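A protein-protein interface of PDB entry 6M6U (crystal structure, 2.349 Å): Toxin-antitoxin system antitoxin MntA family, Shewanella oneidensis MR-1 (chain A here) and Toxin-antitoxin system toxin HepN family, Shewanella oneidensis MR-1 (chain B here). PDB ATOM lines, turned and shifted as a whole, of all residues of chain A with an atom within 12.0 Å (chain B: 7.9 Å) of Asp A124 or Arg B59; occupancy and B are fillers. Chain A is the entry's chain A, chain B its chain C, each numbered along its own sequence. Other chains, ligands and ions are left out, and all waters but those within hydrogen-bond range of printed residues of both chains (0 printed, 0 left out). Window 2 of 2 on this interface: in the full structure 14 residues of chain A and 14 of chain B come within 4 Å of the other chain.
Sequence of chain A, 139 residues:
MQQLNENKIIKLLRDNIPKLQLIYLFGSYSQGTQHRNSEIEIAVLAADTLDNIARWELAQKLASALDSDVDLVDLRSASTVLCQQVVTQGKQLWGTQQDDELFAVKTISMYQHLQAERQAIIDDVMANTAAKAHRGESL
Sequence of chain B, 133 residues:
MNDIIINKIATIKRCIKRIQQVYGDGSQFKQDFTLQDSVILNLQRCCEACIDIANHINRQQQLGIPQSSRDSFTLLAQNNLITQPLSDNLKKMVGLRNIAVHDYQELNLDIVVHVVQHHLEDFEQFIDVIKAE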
ATOM      1  N   LEU A 114     -11.610  23.168  -5.468  1.00  0.00           N
ATOM      2  CA  LEU A 114     -12.613  24.114  -5.943  1.00  0.00           C
ATOM      3  C   LEU A 114     -13.563  23.454  -6.935  1.00  0.00           C
ATOM      4  O   LEU A 114     -14.780  23.651  -6.856  1.00  0.00           O
ATOM      5  CB  LEU A 114     -11.941  25.333  -6.571  1.00  0.00           C
ATOM      6  CG  LEU A 114     -12.929  26.287  -7.248  1.00  0.00           C
ATOM      7  CD1 LEU A 114     -13.846  26.936  -6.212  1.00  0.00           C
ATOM      8  CD2 LEU A 114     -12.193  27.336  -8.070  1.00  0.00           C
ATOM      9  N   GLN A 115     -13.027  22.659  -7.866  1.00  0.00           N
ATOM     10  CA  GLN A 115     -13.878  22.008  -8.857  1.00  0.00           C
ATOM     11  C   GLN A 115     -14.941  21.141  -8.196  1.00  0.00           C
ATOM     12  O   GLN A 115     -16.086  21.091  -8.661  1.00  0.00           O
ATOM     13  CB  GLN A 115     -13.030  21.180  -9.823  1.00  0.00           C
ATOM     14  CG  GLN A 115     -12.237  22.006 -10.836  1.00  0.00           C
ATOM     15  CD  GLN A 115     -13.124  22.734 -11.851  1.00  0.00           C
ATOM     16  OE1 GLN A 115     -13.885  23.644 -11.501  1.00  0.00           O
ATOM     17  NE2 GLN A 115     -13.029  22.328 -13.115  1.00  0.00           N
ATOM     18  N   ALA A 116     -14.591  20.462  -7.100  1.00  0.00           N
ATOM     19  CA  ALA A 116     -15.578  19.669  -6.374  1.00  0.00           C
ATOM     20  C   ALA A 116     -16.687  20.552  -5.807  1.00  0.00           C
ATOM     21  O   ALA A 116     -17.876  20.260  -5.981  1.00  0.00           O
ATOM     22  CB  ALA A 116     -14.900  18.872  -5.260  1.00  0.00           C
ATOM     23  N   GLU A 117     -16.315  21.645  -5.134  1.00  0.00           N
ATOM     24  CA  GLU A 117     -17.315  22.498  -4.494  1.00  0.00           C
ATOM     25  C   GLU A 117     -18.278  23.102  -5.509  1.00  0.00           C
ATOM     26  O   GLU A 117     -19.481  23.200  -5.247  1.00  0.00           O
ATOM     27  CB  GLU A 117     -16.638  23.617  -3.699  1.00  0.00           C
ATOM     28  CG  GLU A 117     -15.529  23.152  -2.780  1.00  0.00           C
ATOM     29  CD  GLU A 117     -14.724  24.299  -2.201  1.00  0.00           C
ATOM     30  OE1 GLU A 117     -14.873  25.446  -2.683  1.00  0.00           O
ATOM     31  OE2 GLU A 117     -13.927  24.045  -1.267  1.00  0.00           O
ATOM     32  N   ARG A 118     -17.771  23.506  -6.674  1.00  0.00           N
ATOM     33  CA  ARG A 118     -18.506  24.368  -7.586  1.00  0.00           C
ATOM     34  C   ARG A 118     -19.050  23.652  -8.819  1.00  0.00           C
ATOM     35  O   ARG A 118     -19.656  24.311  -9.673  1.00  0.00           O
ATOM     36  CB  ARG A 118     -17.608  25.531  -8.030  1.00  0.00           C
ATOM     37  CG  ARG A 118     -16.497  25.108  -8.987  1.00  0.00           C
ATOM     38  CD  ARG A 118     -15.771  26.304  -9.563  1.00  0.00           C
ATOM     39  NE  ARG A 118     -14.854  25.922 -10.633  1.00  0.00           N
ATOM     40  CZ  ARG A 118     -14.386  26.775 -11.538  1.00  0.00           C
ATOM     41  NH1 ARG A 118     -14.754  28.047 -11.493  1.00  0.00           N
ATOM     42  NH2 ARG A 118     -13.559  26.359 -12.488  1.00  0.00           N
ATOM     43  N   GLN A 119     -18.872  22.330  -8.943  1.00  0.00           N
ATOM     44  CA  GLN A 119     -19.199  21.660 -10.206  1.00  0.00           C
ATOM     45  C   GLN A 119     -20.699  21.639 -10.472  1.00  0.00           C
ATOM     46  O   GLN A 119     -21.117  21.580 -11.635  1.00  0.00           O
ATOM     47  CB  GLN A 119     -18.633  20.235 -10.240  1.00  0.00           C
ATOM     48  CG  GLN A 119     -18.601  19.580 -11.632  1.00  0.00           C
ATOM     49  CD  GLN A 119     -17.486  20.134 -12.529  1.00  0.00           C
ATOM     50  OE1 GLN A 119     -16.550  20.779 -12.042  1.00  0.00           O
ATOM     51  NE2 GLN A 119     -17.586  19.867 -13.841  1.00  0.00           N
ATOM     52  N   ALA A 120     -21.527  21.693  -9.425  1.00  0.00           N
ATOM     53  CA  ALA A 120     -22.962  21.823  -9.659  1.00  0.00           C
ATOM     54  C   ALA A 120     -23.309  23.192 -10.244  1.00  0.00           C
ATOM     55  O   ALA A 120     -24.234  23.307 -11.059  1.00  0.00           O
ATOM     56  CB  ALA A 120     -23.730  21.577  -8.363  1.00  0.00           C
ATOM     57  N   ILE A 121     -22.578  24.235  -9.847  1.00  0.00           N
ATOM     58  CA  ILE A 121     -22.853  25.570 -10.363  1.00  0.00           C
ATOM     59  C   ILE A 121     -22.567  25.641 -11.860  1.00  0.00           C
ATOM     60  O   ILE A 121     -23.369  26.182 -12.632  1.00  0.00           O
ATOM     61  CB  ILE A 121     -22.046  26.618  -9.578  1.00  0.00           C
ATOM     62  CG1 ILE A 121     -22.595  26.753  -8.160  1.00  0.00           C
ATOM     63  CG2 ILE A 121     -22.038  27.949 -10.310  1.00  0.00           C
ATOM     64  CD1 ILE A 121     -21.702  27.544  -7.236  1.00  0.00           C
ATOM     65  N   ILE A 122     -21.437  25.083 -12.301  1.00  0.00           N
ATOM     66  CA  ILE A 122     -21.067  25.207 -13.710  1.00  0.00           C
ATOM     67  C   ILE A 122     -21.881  24.233 -14.566  1.00  0.00           C
ATOM     68  O   ILE A 122     -22.202  24.519 -15.728  1.00  0.00           O
ATOM     69  CB  ILE A 122     -19.550  25.001 -13.894  1.00  0.00           C
ATOM     70  CG1 ILE A 122     -19.089  23.698 -13.287  1.00  0.00           C
ATOM     71  CG2 ILE A 122     -18.739  26.138 -13.276  1.00  0.00           C
ATOM     72  CD1 ILE A 122     -19.011  22.571 -14.286  1.00  0.00           C
ATOM     73  N   ASP A 123     -22.207  23.050 -14.018  1.00  0.00           N
ATOM     74  CA  ASP A 123     -23.167  22.178 -14.700  1.00  0.00           C
ATOM     75  C   ASP A 123     -24.484  22.907 -14.946  1.00  0.00           C
ATOM     76  O   ASP A 123     -25.044  22.853 -16.046  1.00  0.00           O
ATOM     77  CB  ASP A 123     -23.423  20.912 -13.884  1.00  0.00           C
ATOM     78  CG  ASP A 123     -22.260  19.929 -13.932  1.00  0.00           C
ATOM     79  OD1 ASP A 123     -21.283  20.175 -14.664  1.00  0.00           O
ATOM     80  OD2 ASP A 123     -22.345  18.870 -13.259  1.00  0.00           O
ATOM     81  N   ASP A 124     -24.992  23.592 -13.917  1.00  0.00           N
ATOM     82  CA  ASP A 124     -26.239  24.342 -14.032  1.00  0.00           C
ATOM     83  C   ASP A 124     -26.116  25.478 -15.048  1.00  0.00           C
ATOM     84  O   ASP A 124     -27.057  25.748 -15.805  1.00  0.00           O
ATOM     85  CB  ASP A 124     -26.628  24.871 -12.652  1.00  0.00           C
ATOM     86  CG  ASP A 124     -27.845  25.768 -12.682  1.00  0.00           C
ATOM     87  OD1 ASP A 124     -27.682  26.990 -12.893  1.00  0.00           O
ATOM     88  OD2 ASP A 124     -28.964  25.253 -12.480  1.00  0.00           O
ATOM     89  N   VAL A 125     -24.961  26.149 -15.083  1.00  0.00           N
ATOM     90  CA  VAL A 125     -24.783  27.297 -15.971  1.00  0.00           C
ATOM     91  C   VAL A 125     -24.558  26.845 -17.412  1.00  0.00           C
ATOM     92  O   VAL A 125     -24.916  27.558 -18.359  1.00  0.00           O
ATOM     93  CB  VAL A 125     -23.630  28.179 -15.445  1.00  0.00           C
ATOM     94  CG1 VAL A 125     -22.973  28.984 -16.567  1.00  0.00           C
ATOM     95  CG2 VAL A 125     -24.137  29.112 -14.351  1.00  0.00           C
ATOM     96  N   MET A 126     -23.990  25.657 -17.610  1.00  0.00           N
ATOM     97  CA  MET A 126     -23.698  25.137 -18.937  1.00  0.00           C
ATOM     98  C   MET A 126     -24.860  24.338 -19.530  1.00  0.00           C
ATOM     99  O   MET A 126     -24.631  23.502 -20.412  1.00  0.00           O
ATOM    100  CB  MET A 126     -22.434  24.276 -18.895  1.00  0.00           C
ATOM    101  CG  MET A 126     -21.121  25.056 -18.794  1.00  0.00           C
ATOM    102  SD  MET A 126     -20.974  26.494 -19.886  1.00  0.00           S
ATOM    103  CE  MET A 126     -19.936  25.820 -21.182  1.00  0.00           C
ATOM    104  N   ALA A 127     -26.087  24.577 -19.067  1.00  0.00           N
ATOM    105  CA  ALA A 127     -27.285  23.889 -19.564  1.00  0.00           C
ATOM    106  C   ALA A 127     -27.162  22.368 -19.482  1.00  0.00           C
ATOM    107  O   ALA A 127     -26.370  21.835 -18.703  1.00  0.00           O
ATOM    108  CB  ALA A 127     -27.591  24.316 -20.999  1.00  0.00           C
ATOM    109  N   ASN B   2     -33.426  23.170  -0.752  1.00  0.00           N
ATOM    110  CA  ASN B   2     -33.463  23.614   0.637  1.00  0.00           C
ATOM    111  C   ASN B   2     -33.337  22.419   1.587  1.00  0.00           C
ATOM    112  O   ASN B   2     -33.018  22.577   2.766  1.00  0.00           O
ATOM    113  CB  ASN B   2     -34.746  24.411   0.908  1.00  0.00           C
ATOM    114  CG  ASN B   2     -35.002  24.632   2.387  1.00  0.00           C
ATOM    115  OD1 ASN B   2     -35.627  23.805   3.049  1.00  0.00           O
ATOM    116  ND2 ASN B   2     -34.504  25.745   2.915  1.00  0.00           N
ATOM    117  N   ILE B   4     -30.978  20.249   1.206  1.00  0.00           N
ATOM    118  CA  ILE B   4     -29.537  20.165   1.416  1.00  0.00           C
ATOM    119  C   ILE B   4     -29.074  21.213   2.423  1.00  0.00           C
ATOM    120  O   ILE B   4     -28.147  20.964   3.203  1.00  0.00           O
ATOM    121  CB  ILE B   4     -28.801  20.304   0.069  1.00  0.00           C
ATOM    122  CG1 ILE B   4     -27.283  20.162   0.253  1.00  0.00           C
ATOM    123  CG2 ILE B   4     -29.142  21.629  -0.595  1.00  0.00           C
ATOM    124  CD1 ILE B   4     -26.826  18.753   0.578  1.00  0.00           C
ATOM    125  N   ASP B  52     -20.677  24.847   1.016  1.00  0.00           N
ATOM    126  CA  ASP B  52     -21.743  24.160   0.293  1.00  0.00           C
ATOM    127  C   ASP B  52     -23.056  24.934   0.372  1.00  0.00           C
ATOM    128  O   ASP B  52     -23.799  25.011  -0.613  1.00  0.00           O
ATOM    129  CB  ASP B  52     -21.921  22.744   0.837  1.00  0.00           C
ATOM    130  CG  ASP B  52     -20.718  21.856   0.569  1.00  0.00           C
ATOM    131  OD1 ASP B  52     -19.865  22.236  -0.264  1.00  0.00           O
ATOM    132  OD2 ASP B  52     -20.636  20.771   1.183  1.00  0.00           O
ATOM    133  N   ILE B  53     -23.362  25.506   1.540  1.00  0.00           N
ATOM    134  CA  ILE B  53     -24.563  26.326   1.678  1.00  0.00           C
ATOM    135  C   ILE B  53     -24.507  27.505   0.715  1.00  0.00           C
ATOM    136  O   ILE B  53     -25.461  27.774  -0.024  1.00  0.00           O
ATOM    137  CB  ILE B  53     -24.731  26.799   3.135  1.00  0.00           C
ATOM    138  CG1 ILE B  53     -25.125  25.629   4.041  1.00  0.00           C
ATOM    139  CG2 ILE B  53     -25.756  27.926   3.222  1.00  0.00           C
ATOM    140  CD1 ILE B  53     -25.254  26.010   5.499  1.00  0.00           C
ATOM    141  N   ALA B  54     -23.375  28.215   0.705  1.00  0.00           N
ATOM    142  CA  ALA B  54     -23.220  29.371  -0.171  1.00  0.00           C
ATOM    143  C   ALA B  54     -23.371  28.983  -1.636  1.00  0.00           C
ATOM    144  O   ALA B  54     -24.048  29.679  -2.402  1.00  0.00           O
ATOM    145  CB  ALA B  54     -21.862  30.029   0.069  1.00  0.00           C
ATOM    146  N   ASN B  55     -22.749  27.872  -2.043  1.00  0.00           N
ATOM    147  CA  ASN B  55     -22.828  27.455  -3.439  1.00  0.00           C
ATOM    148  C   ASN B  55     -24.223  26.984  -3.810  1.00  0.00           C
ATOM    149  O   ASN B  55     -24.639  27.140  -4.963  1.00  0.00           O
ATOM    150  CB  ASN B  55     -21.811  26.351  -3.731  1.00  0.00           C
ATOM    151  CG  ASN B  55     -20.408  26.882  -3.842  1.00  0.00           C
ATOM    152  OD1 ASN B  55     -20.206  28.082  -4.015  1.00  0.00           O
ATOM    153  ND2 ASN B  55     -19.424  25.994  -3.744  1.00  0.00           N
ATOM    154  N   HIS B  56     -24.951  26.388  -2.866  1.00  0.00           N
ATOM    155  CA  HIS B  56     -26.327  26.011  -3.155  1.00  0.00           C
ATOM    156  C   HIS B  56     -27.165  27.238  -3.473  1.00  0.00           C
ATOM    157  O   HIS B  56     -28.018  27.205  -4.367  1.00  0.00           O
ATOM    158  CB  HIS B  56     -26.936  25.241  -1.984  1.00  0.00           C
ATOM    159  CG  HIS B  56     -28.356  24.837  -2.219  1.00  0.00           C
ATOM    160  ND1 HIS B  56     -28.700  23.768  -3.018  1.00  0.00           N
ATOM    161  CD2 HIS B  56     -29.520  25.381  -1.795  1.00  0.00           C
ATOM    162  CE1 HIS B  56     -30.017  23.661  -3.061  1.00  0.00           C
ATOM    163  NE2 HIS B  56     -30.538  24.625  -2.324  1.00  0.00           N
ATOM    164  N   ILE B  57     -26.923  28.338  -2.760  1.00  0.00           N
ATOM    165  CA  ILE B  57     -27.652  29.573  -3.016  1.00  0.00           C
ATOM    166  C   ILE B  57     -27.133  30.249  -4.278  1.00  0.00           C
ATOM    167  O   ILE B  57     -27.913  30.791  -5.072  1.00  0.00           O
ATOM    168  CB  ILE B  57     -27.558  30.494  -1.789  1.00  0.00           C
ATOM    169  CG1 ILE B  57     -28.005  29.725  -0.548  1.00  0.00           C
ATOM    170  CG2 ILE B  57     -28.393  31.741  -1.987  1.00  0.00           C
ATOM    171  CD1 ILE B  57     -27.839  30.490   0.715  1.00  0.00           C
ATOM    172  N   ASN B  58     -25.811  30.231  -4.484  1.00  0.00           N
ATOM    173  CA  ASN B  58     -25.244  30.742  -5.728  1.00  0.00           C
ATOM    174  C   ASN B  58     -25.845  30.038  -6.936  1.00  0.00           C
ATOM    175  O   ASN B  58     -26.132  30.676  -7.954  1.00  0.00           O
ATOM    176  CB  ASN B  58     -23.722  30.575  -5.732  1.00  0.00           C
ATOM    177  CG  ASN B  58     -23.030  31.467  -4.719  1.00  0.00           C
ATOM    178  OD1 ASN B  58     -23.511  32.554  -4.400  1.00  0.00           O
ATOM    179  ND2 ASN B  58     -21.885  31.015  -4.215  1.00  0.00           N
ATOM    180  N   ARG B  59     -26.043  28.720  -6.842  1.00  0.00           N
ATOM    181  CA  ARG B  59     -26.598  27.978  -7.971  1.00  0.00           C
ATOM    182  C   ARG B  59     -28.080  28.273  -8.152  1.00  0.00           C
ATOM    183  O   ARG B  59     -28.543  28.488  -9.278  1.00  0.00           O
ATOM    184  CB  ARG B  59     -26.377  26.476  -7.787  1.00  0.00           C
ATOM    185  CG  ARG B  59     -26.699  25.661  -9.032  1.00  0.00           C
ATOM    186  CD  ARG B  59     -27.617  24.480  -8.741  1.00  0.00           C
ATOM    187  NE  ARG B  59     -27.039  23.547  -7.779  1.00  0.00           N
ATOM    188  CZ  ARG B  59     -27.554  23.297  -6.579  1.00  0.00           C
ATOM    189  NH1 ARG B  59     -28.669  23.907  -6.197  1.00  0.00           N
ATOM    190  NH2 ARG B  59     -26.961  22.432  -5.763  1.00  0.00           N
ATOM    191  N   GLN B  60     -28.840  28.286  -7.054  1.00  0.00           N
ATOM    192  CA  GLN B  60     -30.284  28.470  -7.158  1.00  0.00           C
ATOM    193  C   GLN B  60     -30.636  29.864  -7.662  1.00  0.00           C
ATOM    194  O   GLN B  60     -31.596  30.029  -8.422  1.00  0.00           O
ATOM    195  CB  GLN B  60     -30.946  28.200  -5.807  1.00  0.00           C
ATOM    196  CG  GLN B  60     -31.882  27.003  -5.812  1.00  0.00           C
ATOM    197  CD  GLN B  60     -32.497  26.729  -4.452  1.00  0.00           C
ATOM    198  OE1 GLN B  60     -32.499  27.591  -3.573  1.00  0.00           O
ATOM    199  NE2 GLN B  60     -33.027  25.522  -4.274  1.00  0.00           N
ATOM    200  N   GLN B  61     -29.874  30.878  -7.259  1.00  0.00           N
ATOM    201  CA  GLN B  61     -30.144  32.247  -7.668  1.00  0.00           C
ATOM    202  C   GLN B  61     -29.221  32.739  -8.780  1.00  0.00           C
ATOM    203  O   GLN B  61     -29.302  33.912  -9.154  1.00  0.00           O
ATOM    204  CB  GLN B  61     -30.044  33.188  -6.462  1.00  0.00           C
ATOM    205  CG  GLN B  61     -30.925  32.818  -5.276  1.00  0.00           C
ATOM    206  CD  GLN B  61     -31.001  33.938  -4.253  1.00  0.00           C
ATOM    207  OE1 GLN B  61     -30.777  35.104  -4.582  1.00  0.00           O
ATOM    208  NE2 GLN B  61     -31.305  33.589  -3.003  1.00  0.00           N
ATOM    209  N   GLN B  62     -28.348  31.877  -9.307  1.00  0.00           N
ATOM    210  CA  GLN B  62     -27.484  32.202 -10.444  1.00  0.00           C
ATOM    211  C   GLN B  62     -26.690  33.487 -10.207  1.00  0.00           C
ATOM    212  O   GLN B  62     -26.635  34.382 -11.057  1.00  0.00           O
ATOM    213  CB  GLN B  62     -28.300  32.299 -11.734  1.00  0.00           C
ATOM    214  CG  GLN B  62     -28.949  31.001 -12.164  1.00  0.00           C
ATOM    215  CD  GLN B  62     -30.156  31.244 -13.042  1.00  0.00           C
ATOM    216  OE1 GLN B  62     -30.753  32.321 -13.003  1.00  0.00           O
ATOM    217  NE2 GLN B  62     -30.522  30.249 -13.839  1.00  0.00           N
ATOM    218  N   LEU B  63     -26.067  33.575  -9.028  1.00  0.00           N
ATOM    219  CA  LEU B  63     -25.299  34.761  -8.660  1.00  0.00           C
ATOM    220  C   LEU B  63     -23.925  34.801  -9.307  1.00  0.00           C
ATOM    221  O   LEU B  63     -23.296  35.866  -9.325  1.00  0.00           O
ATOM    222  CB  LEU B  63     -25.139  34.850  -7.136  1.00  0.00           C
ATOM    223  CG  LEU B  63     -26.420  34.573  -6.353  1.00  0.00           C
ATOM    224  CD1 LEU B  63     -26.189  34.725  -4.857  1.00  0.00           C
ATOM    225  CD2 LEU B  63     -27.507  35.532  -6.830  1.00  0.00           C
ATOM    226  N   GLY B  64     -23.449  33.681  -9.838  1.00  0.00           N
ATOM    227  CA  GLY B  64     -22.163  33.670 -10.499  1.00  0.00           C
ATOM    228  C   GLY B  64     -21.396  32.377 -10.317  1.00  0.00           C
ATOM    229  O   GLY B  64     -21.841  31.461  -9.617  1.00  0.00           O
ATOM    230  N   PRO B  66     -18.092  30.848  -8.806  1.00  0.00           N
ATOM    231  CA  PRO B  66     -16.962  31.143  -7.920  1.00  0.00           C
ATOM    232  C   PRO B  66     -15.645  30.784  -8.590  1.00  0.00           C
ATOM    233  O   PRO B  66     -15.523  29.749  -9.247  1.00  0.00           O
ATOM    234  CB  PRO B  66     -17.234  30.270  -6.683  1.00  0.00           C
ATOM    235  CG  PRO B  66     -18.191  29.229  -7.137  1.00  0.00           C
ATOM    236  CD  PRO B  66     -19.019  29.866  -8.221  1.00  0.00           C
ATOM    237  N   LEU B  75     -19.820  36.238  -3.419  1.00  0.00           N
ATOM    238  CA  LEU B  75     -21.008  36.383  -4.254  1.00  0.00           C
ATOM    239  C   LEU B  75     -22.251  36.666  -3.421  1.00  0.00           C
ATOM    240  O   LEU B  75     -23.129  37.424  -3.850  1.00  0.00           O
ATOM    241  CB  LEU B  75     -21.206  35.132  -5.107  1.00  0.00           C
ATOM    242  CG  LEU B  75     -20.103  34.903  -6.137  1.00  0.00           C
ATOM    243  CD1 LEU B  75     -20.289  33.558  -6.825  1.00  0.00           C
ATOM    244  CD2 LEU B  75     -20.094  36.046  -7.142  1.00  0.00           C
ATOM    245  N   LEU B  76     -22.351  36.066  -2.232  1.00  0.00           N
ATOM    246  CA  LEU B  76     -23.510  36.328  -1.382  1.00  0.00           C
ATOM    247  C   LEU B  76     -23.446  37.719  -0.767  1.00  0.00           C
ATOM    248  O   LEU B  76     -24.484  38.364  -0.572  1.00  0.00           O
ATOM    249  CB  LEU B  76     -23.626  35.275  -0.287  1.00  0.00           C
ATOM    250  CG  LEU B  76     -23.624  33.800  -0.689  1.00  0.00           C
ATOM    251  CD1 LEU B  76     -23.629  32.969   0.580  1.00  0.00           C
ATOM    252  CD2 LEU B  76     -24.824  33.452  -1.562  1.00  0.00           C
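Among the printed residues, pairs that only touch across the chains: Ile A121 with Gly B64 (3.6 Å), Ile A121 with Asn B55 (3.6 Å), Ile A121 with Pro B66 (3.7 Å), Asp A124 with Arg B59 (3.7 Å), Ile A121 with Arg B59 (3.8 Å), Ala A120 with Arg B59 (3.9 Å) and Ile A121 with Asn B58 (3.9 Å).
Printed residues of chain B within 4 Å of Ala A120: Arg B59. Of the printed residues of chain B, Ile A121 touches Asn B55 (3.6 Å), Asn B58 (3.9 Å), Arg B59 (3.8 Å), Gly B64 (3.6 Å) and Pro B66 (3.7 Å). Of the printed residues of chain B, Asp A124 touches Arg B59. No residue of chain A comes within 4 Å of His B56. Of chain A, only Ile A121 (3.9 Å) comes within 4 Å of Asn B58. Arg B59 touches just these residues of chain A: Ala A120 (3.9 Å), Ile A121 (3.8 Å) and Asp A124 (3.7 Å). No residue of chain A comes within 4 Å of Gln B60. No residue of chain A comes within 4 Å of Gln B62. The nearest residue of chain A that does not touch Arg B59 is Ile A122 (6.2 Å).
OE1 of Gln A115 sits at hydrogen-bond distance from NE of Arg A118 (2.6 Å). O of Ala B54 sits close to ND2 of Asn B58 (3.1 Å). The backbone carbonyl oxygen of Asn B58 lies within hydrogen-bond range of the backbone NH of Leu B63, 3.1 Å away. The guanidinium group (NH1) of Arg B59 lies within hydrogen-bond range of a ring nitrogen (ND1) of His B56 (3.2 Å). The side-chain amide nitrogen of Asn B58 sits at hydrogen-bond distance from the side-chain amide oxygen of Asn B55 (3.4 Å).
Printed residues of chain A that touch a printed residue of chain B: Glu A117, Arg A118, Ala A120, Ile A121 and Asp A124. Hydrophobic or aromatic side chains of chain A that line the printed part of chain B: Ala A120 and Ile A121. Hydrophobic or aromatic side chains of chain B that line the printed part of chain A: Pro B66. Among the printed residues, 9 pairs touch across the chains.
The side-chain amide nitrogen of Asn B55 sits at hydrogen-bond distance from the backbone carbonyl oxygen of Glu A117. NH1 of Arg A118 sits at hydrogen-bond distance from O of Pro B66.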
